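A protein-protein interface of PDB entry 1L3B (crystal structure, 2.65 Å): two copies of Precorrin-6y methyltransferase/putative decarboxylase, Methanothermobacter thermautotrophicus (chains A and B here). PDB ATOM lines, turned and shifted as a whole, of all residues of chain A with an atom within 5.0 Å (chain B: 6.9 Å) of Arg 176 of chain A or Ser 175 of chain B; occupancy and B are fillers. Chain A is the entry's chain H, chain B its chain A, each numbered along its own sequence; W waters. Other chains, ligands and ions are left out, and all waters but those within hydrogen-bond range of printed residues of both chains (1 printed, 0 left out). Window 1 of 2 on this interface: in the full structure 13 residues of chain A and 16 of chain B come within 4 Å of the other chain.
OG of Ser 175 of chain B lies within hydrogen-bond range of O of Arg 176 of chain A (2.9 Å). The backbone NH (N) of Ser 175 of chain B sits at hydrogen-bond distance from the side-chain amide oxygen (OD1) of Asn 177 of chain A, at 2.7 Å. The side-chain amide oxygen (OD1) of Asn 177 of chain B is in hydrogen-bond range of the backbone NH (N) of Ser 175 of chain A, 3.0 Å away.
N of Arg 163 of chain B lies within hydrogen-bond range of O of Val 174 of chain B, 2.6 Å away. The side-chain hydroxyl of Ser 175 of chain A sits at hydrogen-bond distance from the backbone carbonyl oxygen of Ile 161 of chain A (3.4 Å). O of Ile 161 of chain A lies within hydrogen-bond range of N of Arg 176 of chain A (2.9 Å). N of Val 174 of chain A sits at hydrogen-bond distance from O of Arg 163 of chain A (2.9 Å). NH2 of Arg 163 of chain A lies close to NE of Arg 176 of chain A (2.7 Å). NH1 of Arg 176 of chain A is in hydrogen-bond range of O of Val 174 of chain A (2.9 Å).
CA of Val 174 of chain A touches OD1 of Asn 177 of chain B (3.4 Å). Ser 175 of chain A touches Asn 160 of chain B (OG to OD1, 3.5 Å). Ser 175 of chain A touches Arg 176 of chain B. CB of Asn 177 of chain A touches O of Met 173 of chain B, at 3.2 Å. Asn 177 of chain A touches Val 174 of chain B. Met 173 of chain B touches Pro 178 of chain A. Pro 178 of chain A touches Ser 175 of chain B (CD to OG, 3.8 Å).
Arg 163 of chain A touches none of the printed residues of chain B. Of the printed residues of chain B, Ser 175 of chain A touches Asn 160 (3.5 Å), Arg 176 (3.5 Å) and Asn 177 (3.0 Å). Arg 176 of chain A touches just one residue of chain B: Ser 175. Printed residues of chain B within 4 Å of Pro 178 of chain A: Met 173 (3.2 Å) and Ser 175 (3.8 Å). Of the printed residues of chain A, Asn 160 of chain B touches Ser 175. Of chain A, only Arg 176, Asn 177 and Pro 178 come within 4 Å of Ser 175 of chain B. Of the printed residues of chain A, Arg 176 of chain B touches Ser 175 (3.5 Å). Printed residues of chain A within 4 Å of Asn 177 of chain B: Val 174 and Ser 175. The nearest residue of chain A that does not touch Ser 175 of chain B is Ser 175 of chain A (4.1 Å).
Of the 9 printed residues of chain A, 5 touch a printed residue of chain B. Printed residues of chain A that touch a printed residue of chain B: Val 174, Ser 175, Arg 176, Asn 177 and Pro 178. Hydrophobic or aromatic side chains of chain A within 4 Å of the printed part of chain B: Val 174 and Pro 178. Hydrophobic or aromatic side chains of chain B within 4 Å of the printed part of chain A: Val 174. Among the printed residues, 10 pairs touch across the chains.
Val 174 of chain A touches Asn 177 of chain B, and with the chains exchanged Asn 177 of chain A touches Val 174 of chain B. Ser 175 of chain A touches Asn 160 of chain B, but with the chains exchanged Asn 160 of chain A does not touch Ser 175 of chain B (4.7 Å). Ser 175 of chain A touches Arg 176 of chain B, and with the chains exchanged Arg 176 of chain A touches Ser 175 of chain B. Ser 175 of chain A touches Asn 177 of chain B, and with the chains exchanged Asn 177 of chain A touches Ser 175 of chain B.
Water W1 lies within hydrogen-bond range of O of Met 173 of chain B (2.7 Å) and O of Pro 178 of chain A (3.4 Å).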
ATOM      1  N   ASN A 160      14.827 -14.666   2.771  1.00  0.00           N
ATOM      2  CA  ASN A 160      15.453 -14.976   4.056  1.00  0.00           C
ATOM      3  C   ASN A 160      16.060 -16.307   3.670  1.00  0.00           C
ATOM      4  O   ASN A 160      15.362 -17.302   3.462  1.00  0.00           O
ATOM      5  CB  ASN A 160      14.447 -15.173   5.183  1.00  0.00           C
ATOM      6  CG  ASN A 160      14.297 -13.953   6.055  1.00  0.00           C
ATOM      7  OD1 ASN A 160      15.212 -13.571   6.788  1.00  0.00           O
ATOM      8  ND2 ASN A 160      13.127 -13.330   5.986  1.00  0.00           N
ATOM      9  N   ILE A 161      17.376 -16.305   3.542  1.00  0.00           N
ATOM     10  CA  ILE A 161      18.100 -17.494   3.162  1.00  0.00           C
ATOM     11  C   ILE A 161      18.946 -18.025   4.305  1.00  0.00           C
ATOM     12  O   ILE A 161      19.474 -17.252   5.094  1.00  0.00           O
ATOM     13  CB  ILE A 161      19.016 -17.177   2.003  1.00  0.00           C
ATOM     14  CG1 ILE A 161      18.219 -16.506   0.882  1.00  0.00           C
ATOM     15  CG2 ILE A 161      19.664 -18.442   1.523  1.00  0.00           C
ATOM     16  CD1 ILE A 161      19.130 -15.831  -0.149  1.00  0.00           C
ATOM     17  N   ALA A 162      19.053 -19.353   4.380  1.00  0.00           N
ATOM     18  CA  ALA A 162      19.828 -20.054   5.398  1.00  0.00           C
ATOM     19  C   ALA A 162      20.623 -21.169   4.705  1.00  0.00           C
ATOM     20  O   ALA A 162      20.042 -22.031   4.054  1.00  0.00           O
ATOM     21  CB  ALA A 162      18.914 -20.637   6.422  1.00  0.00           C
ATOM     22  N   ARG A 163      21.946 -21.148   4.839  1.00  0.00           N
ATOM     23  CA  ARG A 163      22.791 -22.159   4.217  1.00  0.00           C
ATOM     24  C   ARG A 163      23.340 -23.058   5.300  1.00  0.00           C
ATOM     25  O   ARG A 163      23.444 -22.649   6.454  1.00  0.00           O
ATOM     26  CB  ARG A 163      23.909 -21.494   3.435  1.00  0.00           C
ATOM     27  CG  ARG A 163      23.391 -20.586   2.340  1.00  0.00           C
ATOM     28  CD  ARG A 163      24.503 -20.120   1.423  1.00  0.00           C
ATOM     29  NE  ARG A 163      24.838 -18.722   1.661  1.00  0.00           N
ATOM     30  CZ  ARG A 163      25.250 -17.871   0.723  1.00  0.00           C
ATOM     31  NH1 ARG A 163      25.379 -18.279  -0.531  1.00  0.00           N
ATOM     32  NH2 ARG A 163      25.524 -16.605   1.038  1.00  0.00           N
ATOM     33  N   VAL A 174      22.938 -21.482   9.024  1.00  0.00           N
ATOM     34  CA  VAL A 174      23.380 -20.105   9.141  1.00  0.00           C
ATOM     35  C   VAL A 174      22.554 -19.194   8.250  1.00  0.00           C
ATOM     36  O   VAL A 174      22.507 -19.363   7.033  1.00  0.00           O
ATOM     37  CB  VAL A 174      24.891 -19.948   8.795  1.00  0.00           C
ATOM     38  CG1 VAL A 174      25.353 -18.537   9.134  1.00  0.00           C
ATOM     39  CG2 VAL A 174      25.716 -20.956   9.585  1.00  0.00           C
ATOM     40  N   SER A 175      21.937 -18.200   8.871  1.00  0.00           N
ATOM     41  CA  SER A 175      21.102 -17.246   8.160  1.00  0.00           C
ATOM     42  C   SER A 175      21.730 -15.954   7.637  1.00  0.00           C
ATOM     43  O   SER A 175      22.452 -15.269   8.350  1.00  0.00           O
ATOM     44  CB  SER A 175      19.922 -16.859   9.047  1.00  0.00           C
ATOM     45  OG  SER A 175      18.686 -17.077   8.360  1.00  0.00           O
ATOM     46  N   ARG A 176      21.465 -15.620   6.380  1.00  0.00           N
ATOM     47  CA  ARG A 176      22.007 -14.388   5.812  1.00  0.00           C
ATOM     48  C   ARG A 176      20.941 -13.381   6.230  1.00  0.00           C
ATOM     49  O   ARG A 176      19.840 -13.783   6.582  1.00  0.00           O
ATOM     50  CB  ARG A 176      22.051 -14.461   4.280  1.00  0.00           C
ATOM     51  CG  ARG A 176      22.734 -15.689   3.725  1.00  0.00           C
ATOM     52  CD  ARG A 176      24.233 -15.564   3.845  1.00  0.00           C
ATOM     53  NE  ARG A 176      24.939 -16.839   3.691  1.00  0.00           N
ATOM     54  CZ  ARG A 176      25.047 -17.764   4.646  1.00  0.00           C
ATOM     55  NH1 ARG A 176      24.491 -17.570   5.832  1.00  0.00           N
ATOM     56  NH2 ARG A 176      25.747 -18.874   4.436  1.00  0.00           N
ATOM     57  N   ASN A 177      21.242 -12.090   6.230  1.00  0.00           N
ATOM     58  CA  ASN A 177      20.210 -11.127   6.617  1.00  0.00           C
ATOM     59  C   ASN A 177      19.155 -11.011   5.518  1.00  0.00           C
ATOM     60  O   ASN A 177      19.425 -11.281   4.340  1.00  0.00           O
ATOM     61  CB  ASN A 177      20.789  -9.737   6.845  1.00  0.00           C
ATOM     62  CG  ASN A 177      21.677  -9.671   8.046  1.00  0.00           C
ATOM     63  OD1 ASN A 177      21.330 -10.164   9.122  1.00  0.00           O
ATOM     64  ND2 ASN A 177      22.831  -9.041   7.882  1.00  0.00           N
ATOM     65  N   PRO A 178      17.947 -10.568   5.884  1.00  0.00           N
ATOM     66  CA  PRO A 178      16.873 -10.426   4.896  1.00  0.00           C
ATOM     67  C   PRO A 178      17.295  -9.605   3.669  1.00  0.00           C
ATOM     68  O   PRO A 178      18.128  -8.706   3.769  1.00  0.00           O
ATOM     69  CB  PRO A 178      15.773  -9.742   5.697  1.00  0.00           C
ATOM     70  CG  PRO A 178      16.012 -10.243   7.110  1.00  0.00           C
ATOM     71  CD  PRO A 178      17.509 -10.128   7.225  1.00  0.00           C
ATOM     72  N   ASN B 160      12.595 -17.704  12.740  1.00  0.00           N
ATOM     73  CA  ASN B 160      13.660 -16.991  12.038  1.00  0.00           C
ATOM     74  C   ASN B 160      13.401 -15.588  12.533  1.00  0.00           C
ATOM     75  O   ASN B 160      12.312 -15.050  12.357  1.00  0.00           O
ATOM     76  CB  ASN B 160      13.484 -17.043  10.530  1.00  0.00           C
ATOM     77  CG  ASN B 160      14.332 -18.111   9.890  1.00  0.00           C
ATOM     78  OD1 ASN B 160      15.547 -17.953   9.726  1.00  0.00           O
ATOM     79  ND2 ASN B 160      13.703 -19.219   9.543  1.00  0.00           N
ATOM     80  N   ILE B 161      14.387 -14.995  13.176  1.00  0.00           N
ATOM     81  CA  ILE B 161      14.211 -13.658  13.698  1.00  0.00           C
ATOM     82  C   ILE B 161      15.109 -12.648  13.041  1.00  0.00           C
ATOM     83  O   ILE B 161      16.183 -12.993  12.550  1.00  0.00           O
ATOM     84  CB  ILE B 161      14.478 -13.653  15.200  1.00  0.00           C
ATOM     85  CG1 ILE B 161      13.598 -14.706  15.883  1.00  0.00           C
ATOM     86  CG2 ILE B 161      14.230 -12.271  15.761  1.00  0.00           C
ATOM     87  CD1 ILE B 161      13.882 -14.849  17.359  1.00  0.00           C
ATOM     88  N   ALA B 162      14.644 -11.403  12.998  1.00  0.00           N
ATOM     89  CA  ALA B 162      15.398 -10.295  12.403  1.00  0.00           C
ATOM     90  C   ALA B 162      15.213  -9.066  13.306  1.00  0.00           C
ATOM     91  O   ALA B 162      14.092  -8.671  13.616  1.00  0.00           O
ATOM     92  CB  ALA B 162      14.884  -9.991  11.008  1.00  0.00           C
ATOM     93  N   ARG B 163      16.308  -8.482  13.757  1.00  0.00           N
ATOM     94  CA  ARG B 163      16.217  -7.314  14.608  1.00  0.00           C
ATOM     95  C   ARG B 163      16.751  -6.139  13.790  1.00  0.00           C
ATOM     96  O   ARG B 163      17.510  -6.331  12.832  1.00  0.00           O
ATOM     97  CB  ARG B 163      17.013  -7.520  15.895  1.00  0.00           C
ATOM     98  CG  ARG B 163      16.542  -8.716  16.750  1.00  0.00           C
ATOM     99  CD  ARG B 163      16.751  -8.472  18.242  1.00  0.00           C
ATOM    100  NE  ARG B 163      17.240  -9.656  18.931  1.00  0.00           N
ATOM    101  CZ  ARG B 163      18.508 -10.062  18.907  1.00  0.00           C
ATOM    102  NH1 ARG B 163      19.411  -9.365  18.224  1.00  0.00           N
ATOM    103  NH2 ARG B 163      18.884 -11.165  19.558  1.00  0.00           N
ATOM    104  N   MET B 173      18.016  -4.802   8.716  1.00  0.00           N
ATOM    105  CA  MET B 173      17.457  -5.960   9.382  1.00  0.00           C
ATOM    106  C   MET B 173      18.530  -7.037   9.471  1.00  0.00           C
ATOM    107  O   MET B 173      19.014  -7.547   8.457  1.00  0.00           O
ATOM    108  CB  MET B 173      16.208  -6.513   8.662  1.00  0.00           C
ATOM    109  CG  MET B 173      14.999  -5.533   8.564  1.00  0.00           C
ATOM    110  SD  MET B 173      14.596  -4.581  10.184  1.00  0.00           S
ATOM    111  CE  MET B 173      13.488  -5.910  11.155  1.00  0.00           C
ATOM    112  N   VAL B 174      18.916  -7.356  10.701  1.00  0.00           N
ATOM    113  CA  VAL B 174      19.925  -8.366  10.945  1.00  0.00           C
ATOM    114  C   VAL B 174      19.184  -9.552  11.503  1.00  0.00           C
ATOM    115  O   VAL B 174      18.404  -9.431  12.449  1.00  0.00           O
ATOM    116  CB  VAL B 174      20.963  -7.900  11.981  1.00  0.00           C
ATOM    117  CG1 VAL B 174      22.073  -8.928  12.122  1.00  0.00           C
ATOM    118  CG2 VAL B 174      21.531  -6.563  11.551  1.00  0.00           C
ATOM    119  N   SER B 175      19.427 -10.705  10.912  1.00  0.00           N
ATOM    120  CA  SER B 175      18.763 -11.892  11.373  1.00  0.00           C
ATOM    121  C   SER B 175      19.635 -12.770  12.226  1.00  0.00           C
ATOM    122  O   SER B 175      20.861 -12.711  12.169  1.00  0.00           O
ATOM    123  CB  SER B 175      18.272 -12.682  10.185  1.00  0.00           C
ATOM    124  OG  SER B 175      19.321 -12.769   9.265  1.00  0.00           O
ATOM    125  N   ARG B 176      18.965 -13.567  13.046  1.00  0.00           N
ATOM    126  CA  ARG B 176      19.616 -14.499  13.941  1.00  0.00           C
ATOM    127  C   ARG B 176      19.485 -15.816  13.178  1.00  0.00           C
ATOM    128  O   ARG B 176      18.702 -15.918  12.229  1.00  0.00           O
ATOM    129  CB  ARG B 176      18.837 -14.602  15.257  1.00  0.00           C
ATOM    130  CG  ARG B 176      18.687 -13.307  16.039  1.00  0.00           C
ATOM    131  CD  ARG B 176      19.904 -13.007  16.909  1.00  0.00           C
ATOM    132  NE  ARG B 176      20.515 -11.728  16.530  1.00  0.00           N
ATOM    133  CZ  ARG B 176      21.693 -11.608  15.919  1.00  0.00           C
ATOM    134  NH1 ARG B 176      22.401 -12.689  15.619  1.00  0.00           N
ATOM    135  NH2 ARG B 176      22.159 -10.410  15.587  1.00  0.00           N
ATOM    136  N   ASN B 177      20.250 -16.822  13.580  1.00  0.00           N
ATOM    137  CA  ASN B 177      20.175 -18.106  12.915  1.00  0.00           C
ATOM    138  C   ASN B 177      18.885 -18.748  13.371  1.00  0.00           C
ATOM    139  O   ASN B 177      18.439 -18.542  14.497  1.00  0.00           O
ATOM    140  CB  ASN B 177      21.322 -19.005  13.325  1.00  0.00           C
ATOM    141  CG  ASN B 177      22.660 -18.516  12.827  1.00  0.00           C
ATOM    142  OD1 ASN B 177      22.775 -17.949  11.733  1.00  0.00           O
ATOM    143  ND2 ASN B 177      23.699 -18.785  13.609  1.00  0.00           N
HETATM  144  O   HOH W   1      20.026  -7.016   6.012  1.00  0.00           O
